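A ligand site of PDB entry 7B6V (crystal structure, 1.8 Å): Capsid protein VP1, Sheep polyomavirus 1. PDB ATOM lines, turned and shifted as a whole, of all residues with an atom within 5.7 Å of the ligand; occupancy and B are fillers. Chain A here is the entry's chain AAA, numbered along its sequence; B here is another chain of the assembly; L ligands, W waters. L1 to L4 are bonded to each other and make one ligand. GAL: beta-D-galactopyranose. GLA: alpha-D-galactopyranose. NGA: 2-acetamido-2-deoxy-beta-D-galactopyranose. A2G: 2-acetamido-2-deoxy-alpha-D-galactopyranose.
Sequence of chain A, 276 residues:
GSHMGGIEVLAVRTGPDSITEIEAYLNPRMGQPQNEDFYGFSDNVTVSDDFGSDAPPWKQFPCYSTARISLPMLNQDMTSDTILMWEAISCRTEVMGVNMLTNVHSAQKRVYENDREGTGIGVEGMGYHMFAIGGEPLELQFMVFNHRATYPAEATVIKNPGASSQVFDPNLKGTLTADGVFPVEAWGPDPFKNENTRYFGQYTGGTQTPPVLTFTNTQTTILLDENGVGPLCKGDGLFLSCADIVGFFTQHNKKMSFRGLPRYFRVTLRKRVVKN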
ATOM      1  N   GLN A  32      14.785 -21.436  21.228  1.00  0.00           N
ATOM      2  CA  GLN A  32      15.224 -20.686  20.023  1.00  0.00           C
ATOM      3  C   GLN A  32      16.497 -21.342  19.494  1.00  0.00           C
ATOM      4  O   GLN A  32      17.346 -21.799  20.270  1.00  0.00           O
ATOM      5  CB  GLN A  32      15.444 -19.203  20.283  1.00  0.00           C
ATOM      6  CG  GLN A  32      14.166 -18.468  20.658  1.00  0.00           C
ATOM      7  CD  GLN A  32      13.354 -18.125  19.428  1.00  0.00           C
ATOM      8  OE1 GLN A  32      13.273 -18.906  18.491  1.00  0.00           O
ATOM      9  NE2 GLN A  32      12.783 -16.935  19.424  1.00  0.00           N
ATOM     10  N   PHE A  38      18.133 -15.024  19.101  1.00  0.00           N
ATOM     11  CA  PHE A  38      17.348 -15.321  20.329  1.00  0.00           C
ATOM     12  C   PHE A  38      17.933 -16.537  21.043  1.00  0.00           C
ATOM     13  O   PHE A  38      17.269 -17.058  21.976  1.00  0.00           O
ATOM     14  CB  PHE A  38      15.847 -15.395  19.987  1.00  0.00           C
ATOM     15  CG  PHE A  38      15.346 -14.077  19.452  1.00  0.00           C
ATOM     16  CD1 PHE A  38      15.153 -12.990  20.286  1.00  0.00           C
ATOM     17  CD2 PHE A  38      15.205 -13.886  18.084  1.00  0.00           C
ATOM     18  CE1 PHE A  38      14.767 -11.754  19.759  1.00  0.00           C
ATOM     19  CE2 PHE A  38      14.796 -12.657  17.572  1.00  0.00           C
ATOM     20  CZ  PHE A  38      14.605 -11.602  18.409  1.00  0.00           C
ATOM     21  N   ASP A  43      11.021 -18.955  22.257  1.00  0.00           N
ATOM     22  CA  ASP A  43      10.134 -18.074  21.478  1.00  0.00           C
ATOM     23  C   ASP A  43       9.004 -17.642  22.431  1.00  0.00           C
ATOM     24  O   ASP A  43       8.833 -18.213  23.522  1.00  0.00           O
ATOM     25  CB  ASP A  43       9.622 -18.765  20.221  1.00  0.00           C
ATOM     26  CG  ASP A  43       9.189 -17.851  19.079  1.00  0.00           C
ATOM     27  OD1 ASP A  43       9.118 -16.611  19.281  1.00  0.00           O
ATOM     28  OD2 ASP A  43       8.933 -18.391  17.999  1.00  0.00           O
ATOM     29  N   ASN A  44       8.222 -16.650  22.014  1.00  0.00           N
ATOM     30  CA  ASN A  44       7.181 -16.025  22.859  1.00  0.00           C
ATOM     31  C   ASN A  44       6.132 -17.102  23.146  1.00  0.00           C
ATOM     32  O   ASN A  44       5.618 -17.705  22.188  1.00  0.00           O
ATOM     33  CB  ASN A  44       6.731 -14.719  22.204  1.00  0.00           C
ATOM     34  CG  ASN A  44       7.873 -13.731  22.173  1.00  0.00           C
ATOM     35  OD1 ASN A  44       8.372 -13.333  23.242  1.00  0.00           O
ATOM     36  ND2 ASN A  44       8.312 -13.329  20.986  1.00  0.00           N
ATOM     37  N   LYS A  59       9.885 -24.583  19.988  1.00  0.00           N
ATOM     38  CA  LYS A  59      10.646 -23.340  20.347  1.00  0.00           C
ATOM     39  C   LYS A  59      10.058 -22.598  21.569  1.00  0.00           C
ATOM     40  O   LYS A  59      10.796 -21.750  22.101  1.00  0.00           O
ATOM     41  CB  LYS A  59      10.782 -22.357  19.180  1.00  0.00           C
ATOM     42  CG  LYS A  59      11.514 -22.896  17.960  1.00  0.00           C
ATOM     43  CD  LYS A  59      11.750 -21.875  16.896  1.00  0.00           C
ATOM     44  CE  LYS A  59      10.454 -21.374  16.293  1.00  0.00           C
ATOM     45  NZ  LYS A  59      10.709 -20.621  15.050  1.00  0.00           N
ATOM     46  N   GLN A  60       8.834 -22.862  22.007  1.00  0.00           N
ATOM     47  CA  GLN A  60       8.194 -22.086  23.117  1.00  0.00           C
ATOM     48  C   GLN A  60       8.391 -22.723  24.505  1.00  0.00           C
ATOM     49  O   GLN A  60       7.857 -22.182  25.473  1.00  0.00           O
ATOM     50  CB  GLN A  60       6.703 -21.903  22.837  1.00  0.00           C
ATOM     51  CG  GLN A  60       6.451 -21.066  21.588  1.00  0.00           C
ATOM     52  CD  GLN A  60       4.979 -20.852  21.312  1.00  0.00           C
ATOM     53  OE1 GLN A  60       4.108 -21.033  22.171  1.00  0.00           O
ATOM     54  NE2 GLN A  60       4.681 -20.482  20.074  1.00  0.00           N
ATOM     55  N   ALA A 107      15.279  -3.905  25.593  1.00  0.00           N
ATOM     56  CA  ALA A 107      13.910  -4.146  25.071  1.00  0.00           C
ATOM     57  C   ALA A 107      12.954  -4.782  26.097  1.00  0.00           C
ATOM     58  O   ALA A 107      12.154  -5.678  25.738  1.00  0.00           O
ATOM     59  CB  ALA A 107      14.009  -4.975  23.825  1.00  0.00           C
ATOM     60  N   PHE A 249      11.731 -13.216  30.182  1.00  0.00           N
ATOM     61  CA  PHE A 249      12.036 -11.922  29.544  1.00  0.00           C
ATOM     62  C   PHE A 249      10.669 -11.389  29.095  1.00  0.00           C
ATOM     63  O   PHE A 249       9.965 -12.158  28.433  1.00  0.00           O
ATOM     64  CB  PHE A 249      13.018 -12.090  28.393  1.00  0.00           C
ATOM     65  CG  PHE A 249      13.052 -10.952  27.406  1.00  0.00           C
ATOM     66  CD1 PHE A 249      13.099  -9.634  27.820  1.00  0.00           C
ATOM     67  CD2 PHE A 249      13.059 -11.194  26.036  1.00  0.00           C
ATOM     68  CE1 PHE A 249      13.218  -8.600  26.907  1.00  0.00           C
ATOM     69  CE2 PHE A 249      13.079 -10.147  25.123  1.00  0.00           C
ATOM     70  CZ  PHE A 249      13.178  -8.857  25.565  1.00  0.00           C
ATOM     71  N   GLN A 251       8.711  -8.348  27.028  1.00  0.00           N
ATOM     72  CA  GLN A 251       8.864  -7.262  26.029  1.00  0.00           C
ATOM     73  C   GLN A 251       7.868  -6.144  26.346  1.00  0.00           C
ATOM     74  O   GLN A 251       6.973  -6.397  27.171  1.00  0.00           O
ATOM     75  CB  GLN A 251       8.555  -7.754  24.616  1.00  0.00           C
ATOM     76  CG  GLN A 251       9.548  -8.781  24.082  1.00  0.00           C
ATOM     77  CD  GLN A 251       9.385  -9.104  22.600  1.00  0.00           C
ATOM     78  OE1 GLN A 251      10.312  -9.617  21.965  1.00  0.00           O
ATOM     79  NE2 GLN A 251       8.217  -8.828  22.039  1.00  0.00           N
ATOM     80  N   HIS A 252       8.025  -4.962  25.732  1.00  0.00           N
ATOM     81  CA  HIS A 252       7.080  -3.814  25.864  1.00  0.00           C
ATOM     82  C   HIS A 252       5.657  -4.274  25.526  1.00  0.00           C
ATOM     83  O   HIS A 252       4.692  -3.778  26.160  1.00  0.00           O
ATOM     84  CB  HIS A 252       7.508  -2.640  24.956  1.00  0.00           C
ATOM     85  CG  HIS A 252       8.849  -2.079  25.253  1.00  0.00           C
ATOM     86  ND1 HIS A 252       9.081  -1.313  26.364  1.00  0.00           N
ATOM     87  CD2 HIS A 252      10.034  -2.197  24.624  1.00  0.00           C
ATOM     88  CE1 HIS A 252      10.360  -0.970  26.401  1.00  0.00           C
ATOM     89  NE2 HIS A 252      10.952  -1.464  25.314  1.00  0.00           N
ATOM     90  N   ASN A 253       5.491  -5.164  24.547  1.00  0.00           N
ATOM     91  CA  ASN A 253       4.129  -5.620  24.154  1.00  0.00           C
ATOM     92  C   ASN A 253       3.660  -6.737  25.108  1.00  0.00           C
ATOM     93  O   ASN A 253       2.575  -7.246  24.868  1.00  0.00           O
ATOM     94  CB  ASN A 253       4.045  -6.019  22.680  1.00  0.00           C
ATOM     95  CG  ASN A 253       4.968  -7.149  22.277  1.00  0.00           C
ATOM     96  OD1 ASN A 253       5.605  -7.781  23.122  1.00  0.00           O
ATOM     97  ND2 ASN A 253       5.064  -7.398  20.967  1.00  0.00           N
ATOM     98  N   LYS A 255       4.785  -9.693  25.606  1.00  0.00           N
ATOM     99  CA  LYS A 255       5.225 -11.050  25.190  1.00  0.00           C
ATOM    100  C   LYS A 255       6.347 -11.506  26.125  1.00  0.00           C
ATOM    101  O   LYS A 255       7.273 -10.719  26.383  1.00  0.00           O
ATOM    102  CB  LYS A 255       5.652 -11.081  23.719  1.00  0.00           C
ATOM    103  CG  LYS A 255       4.458 -10.998  22.772  1.00  0.00           C
ATOM    104  CD  LYS A 255       4.821 -11.310  21.350  1.00  0.00           C
ATOM    105  CE  LYS A 255       3.735 -10.888  20.386  1.00  0.00           C
ATOM    106  NZ  LYS A 255       2.594 -11.832  20.416  1.00  0.00           N
ATOM    107  N   ASP B  49      13.863  -0.177  22.347  1.00  0.00           N
ATOM    108  CA  ASP B  49      12.578  -0.708  21.846  1.00  0.00           C
ATOM    109  C   ASP B  49      12.773  -2.113  21.251  1.00  0.00           C
ATOM    110  O   ASP B  49      11.782  -2.838  21.116  1.00  0.00           O
ATOM    111  CB  ASP B  49      11.952   0.248  20.830  1.00  0.00           C
ATOM    112  CG  ASP B  49      11.372   1.491  21.481  1.00  0.00           C
ATOM    113  OD1 ASP B  49      11.168   1.483  22.719  1.00  0.00           O
ATOM    114  OD2 ASP B  49      11.129   2.452  20.752  1.00  0.00           O
ATOM    115  N   ASP B  50      13.994  -2.496  20.890  1.00  0.00           N
ATOM    116  CA  ASP B  50      14.290  -3.870  20.409  1.00  0.00           C
ATOM    117  C   ASP B  50      15.775  -4.173  20.588  1.00  0.00           C
ATOM    118  O   ASP B  50      16.556  -3.249  20.846  1.00  0.00           O
ATOM    119  CB  ASP B  50      13.833  -4.078  18.964  1.00  0.00           C
ATOM    120  CG  ASP B  50      14.482  -3.175  17.932  1.00  0.00           C
ATOM    121  OD1 ASP B  50      15.675  -2.845  18.090  1.00  0.00           O
ATOM    122  OD2 ASP B  50      13.819  -2.857  16.939  1.00  0.00           O
ATOM    123  N   PHE B  51      16.155  -5.440  20.432  1.00  0.00           N
ATOM    124  CA  PHE B  51      17.539  -5.923  20.580  1.00  0.00           C
ATOM    125  C   PHE B  51      18.433  -5.276  19.513  1.00  0.00           C
ATOM    126  O   PHE B  51      19.564  -4.947  19.808  1.00  0.00           O
ATOM    127  CB  PHE B  51      17.588  -7.457  20.502  1.00  0.00           C
ATOM    128  CG  PHE B  51      17.259  -8.177  21.793  1.00  0.00           C
ATOM    129  CD1 PHE B  51      16.826  -7.488  22.920  1.00  0.00           C
ATOM    130  CD2 PHE B  51      17.409  -9.571  21.886  1.00  0.00           C
ATOM    131  CE1 PHE B  51      16.528  -8.161  24.103  1.00  0.00           C
ATOM    132  CE2 PHE B  51      17.080 -10.238  23.048  1.00  0.00           C
ATOM    133  CZ  PHE B  51      16.672  -9.528  24.172  1.00  0.00           C
ATOM    134  N   GLY B  52      17.902  -5.040  18.314  1.00  0.00           N
ATOM    135  CA  GLY B  52      18.668  -4.566  17.143  1.00  0.00           C
ATOM    136  C   GLY B  52      19.168  -3.121  17.283  1.00  0.00           C
ATOM    137  O   GLY B  52      20.217  -2.835  16.705  1.00  0.00           O
ATOM    138  N   ARG B 148      23.403  -8.052  20.329  1.00  0.00           N
ATOM    139  CA  ARG B 148      23.311  -6.920  19.355  1.00  0.00           C
ATOM    140  C   ARG B 148      23.420  -5.584  20.081  1.00  0.00           C
ATOM    141  O   ARG B 148      23.550  -4.569  19.393  1.00  0.00           O
ATOM    142  CB  ARG B 148      22.062  -7.050  18.507  1.00  0.00           C
ATOM    143  CG  ARG B 148      22.146  -8.248  17.561  1.00  0.00           C
ATOM    144  CD  ARG B 148      20.932  -8.353  16.712  1.00  0.00           C
ATOM    145  NE  ARG B 148      19.819  -8.948  17.424  1.00  0.00           N
ATOM    146  CZ  ARG B 148      18.546  -8.843  17.070  1.00  0.00           C
ATOM    147  NH1 ARG B 148      18.197  -8.131  16.007  1.00  0.00           N
ATOM    148  NH2 ARG B 148      17.638  -9.462  17.785  1.00  0.00           N
HETATM  149  C1  GAL L   1       2.875 -12.912  12.491  1.00  0.00           C
HETATM  150  C2  GAL L   1       3.995 -13.923  12.638  1.00  0.00           C
HETATM  151  C3  GAL L   1       3.546 -15.176  13.354  1.00  0.00           C
HETATM  152  C4  GAL L   1       2.916 -14.795  14.677  1.00  0.00           C
HETATM  153  C5  GAL L   1       1.769 -13.841  14.400  1.00  0.00           C
HETATM  154  C6  GAL L   1       1.003 -13.466  15.650  1.00  0.00           C
HETATM  155  O1  GAL L   1       3.509 -11.735  12.016  1.00  0.00           O
HETATM  156  O2  GAL L   1       4.511 -14.309  11.362  1.00  0.00           O
HETATM  157  O3  GAL L   1       4.748 -15.931  13.511  1.00  0.00           O
HETATM  158  O4  GAL L   1       3.902 -14.102  15.474  1.00  0.00           O
HETATM  159  O5  GAL L   1       2.252 -12.651  13.751  1.00  0.00           O
HETATM  160  O6  GAL L   1      -0.018 -12.551  15.235  1.00  0.00           O
HETATM  161  C1  GLA L   2       3.935 -14.598  16.803  1.00  0.00           C
HETATM  162  C2  GLA L   2       4.720 -13.519  17.588  1.00  0.00           C
HETATM  163  C3  GLA L   2       6.188 -13.570  17.214  1.00  0.00           C
HETATM  164  C4  GLA L   2       6.730 -15.016  17.265  1.00  0.00           C
HETATM  165  C5  GLA L   2       5.887 -15.908  16.378  1.00  0.00           C
HETATM  166  C6  GLA L   2       6.363 -17.350  16.251  1.00  0.00           C
HETATM  167  O2  GLA L   2       4.205 -12.193  17.363  1.00  0.00           O
HETATM  168  O3  GLA L   2       6.860 -12.721  18.133  1.00  0.00           O
HETATM  169  O4  GLA L   2       6.741 -15.497  18.608  1.00  0.00           O
HETATM  170  O5  GLA L   2       4.534 -15.892  16.843  1.00  0.00           O
HETATM  171  O6  GLA L   2       7.763 -17.470  15.953  1.00  0.00           O
HETATM  172  C1  NGA L   3       8.118 -12.170  17.743  1.00  0.00           C
HETATM  173  C2  NGA L   3       8.356 -10.766  18.306  1.00  0.00           C
HETATM  174  C3  NGA L   3       9.792 -10.293  18.102  1.00  0.00           C
HETATM  175  C4  NGA L   3      10.744 -11.390  18.694  1.00  0.00           C
HETATM  176  C5  NGA L   3      10.470 -12.698  18.019  1.00  0.00           C
HETATM  177  C6  NGA L   3      11.250 -13.869  18.655  1.00  0.00           C
HETATM  178  C7  NGA L   3       6.525  -9.154  18.491  1.00  0.00           C
HETATM  179  C8  NGA L   3       5.672  -8.248  17.710  1.00  0.00           C
HETATM  180  N2  NGA L   3       7.355  -9.886  17.722  1.00  0.00           N
HETATM  181  O3  NGA L   3       9.916  -9.041  18.754  1.00  0.00           O
HETATM  182  O4  NGA L   3      10.383 -11.621  20.084  1.00  0.00           O
HETATM  183  O5  NGA L   3       9.128 -13.066  18.163  1.00  0.00           O
HETATM  184  O6  NGA L   3      11.033 -15.105  17.942  1.00  0.00           O
HETATM  185  O7  NGA L   3       6.522  -9.146  19.718  1.00  0.00           O
HETATM  186  O5  A2G L   4      10.130  -7.431  17.241  1.00  0.00           O
HETATM  187  C1  A2G L   4      10.865  -8.097  18.275  1.00  0.00           C
HETATM  188  C2  A2G L   4      11.278  -7.243  19.449  1.00  0.00           C
HETATM  189  N2  A2G L   4      11.831  -8.113  20.501  1.00  0.00           N
HETATM  190  C3  A2G L   4      10.093  -6.382  19.932  1.00  0.00           C
HETATM  191  O3  A2G L   4      10.533  -5.505  20.934  1.00  0.00           O
HETATM  192  C4  A2G L   4       9.532  -5.598  18.735  1.00  0.00           C
HETATM  193  O4  A2G L   4      10.534  -4.716  18.214  1.00  0.00           O
HETATM  194  C5  A2G L   4       9.054  -6.570  17.662  1.00  0.00           C
HETATM  195  C6  A2G L   4       8.466  -5.835  16.439  1.00  0.00           C
HETATM  196  O6  A2G L   4       7.686  -6.783  15.701  1.00  0.00           O
HETATM  197  C7  A2G L   4      13.133  -8.108  20.732  1.00  0.00           C
HETATM  198  O7  A2G L   4      13.892  -7.477  20.002  1.00  0.00           O
HETATM  199  C8  A2G L   4      13.602  -8.910  21.922  1.00  0.00           C
HETATM  200  O   HOH W   1      11.710 -15.687  15.437  1.00  0.00           O
HETATM  201  O   HOH W   2       7.967 -19.722  14.452  1.00  0.00           O
HETATM  202  O   HOH W   3      12.169 -12.417  22.485  1.00  0.00           O
HETATM  203  O   HOH W   4       7.235 -10.101  14.610  1.00  0.00           O
HETATM  204  O   HOH W   5      11.509 -11.252  15.021  1.00  0.00           O
HETATM  205  O   HOH W   6      14.832  -8.403  17.661  1.00  0.00           O
HETATM  206  O   HOH W   7       3.917 -11.195  15.107  1.00  0.00           O
HETATM  207  O   HOH W   8       1.351 -10.750  18.043  1.00  0.00           O
HETATM  208  O   HOH W   9      10.132  -5.195  23.720  1.00  0.00           O
HETATM  209  O   HOH W  10       7.494  -4.846  22.073  1.00  0.00           O
HETATM  210  O   HOH W  11      11.979  -5.201  16.334  1.00  0.00           O
HETATM  211  O   HOH W  12       3.297 -17.928  18.121  1.00  0.00           O
HETATM  212  O   HOH W  13       9.229  -2.514  21.198  1.00  0.00           O
HETATM  213  O   HOH W  14       3.138 -18.433  14.666  1.00  0.00           O
HETATM  214  O   HOH W  15       4.763 -16.737  19.808  1.00  0.00           O
HETATM  215  O   HOH W  16       9.882  -8.294  14.124  1.00  0.00           O
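The side-chain carboxylate of Asp 43 lies within hydrogen-bond range of an oxygen (O6) of GLA L2, at 2.5 Å. The side-chain amide oxygen (OE1) of Gln 251 sits at hydrogen-bond distance from a nitrogen (N2) of A2G L4 (2.6 Å). The side-chain amide nitrogen (ND2) of Asn 253 is in hydrogen-bond range of an oxygen (O7) of NGA L3 (2.6 Å). An oxygen (O4) of NGA L3 sits at hydrogen-bond distance from the side-chain amide nitrogen (ND2) of Asn 44 (2.8 Å). The side-chain amide nitrogen (NE2) of Gln 32 is in hydrogen-bond range of an oxygen (O6) of NGA L3 (2.9 Å). The backbone carbonyl oxygen of Asp 49 of chain B lies within hydrogen-bond range of an oxygen (O3) of A2G L4 (3.0 Å). The backbone NH (N) of Phe 51 of chain B lies within hydrogen-bond range of an oxygen (O7) of A2G L4 (3.1 Å). NZ of Lys 255 sits close to O2 of GLA L2 (3.5 Å).
Water W6 lies within hydrogen-bond range of an oxygen (O7) of A2G L4 (2.7 Å) and the guanidinium group (NH2) of Arg 148 of chain B (3.0 Å). Water W2 bridges O6 of GLA L2 (2.7 Å) and NZ of Lys 59 (2.9 Å). Water W9 lies within hydrogen-bond range of O3 of A2G L4 (2.8 Å), O of Ala 107 (2.9 Å) and N of His 252 (2.9 Å). Water W8 lies within hydrogen-bond range of NZ of Lys 255 (2.9 Å) and O2 of GLA L2 (3.3 Å). Water W13 bridges the backbone carbonyl oxygen of Asp 49 of chain B (2.6 Å) and an oxygen (O3) of A2G L4 (3.3 Å). Water W10 lies within hydrogen-bond range of N of Asn 253 (3.2 Å) and O3 of A2G L4 (3.3 Å).
Merely in contact with the ligand: Asp 50 of chain B, Phe 249 and Phe 38. Of the 17 residues printed, 11 come within 4 Å of the ligand. The nearest printed residue that does not touch the ligand is Ala 107 (4.4 Å).
The backbone carbonyl oxygen (O) of Lys 59 sits at hydrogen-bond distance from the backbone NH (N) of Asp 43, at 2.8 Å. The side-chain amide oxygen (OD1) of Asn 253 sits at hydrogen-bond distance from the side-chain amide nitrogen (NE2) of Gln 251 (3.0 Å). The backbone NH (N) of Lys 255 lies close to the side-chain amide oxygen (OD1) of Asn 253, 3.2 Å away. N of Gly 52 of chain B lies within hydrogen-bond range of OD1 of Asp 50 of chain B (3.1 Å).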
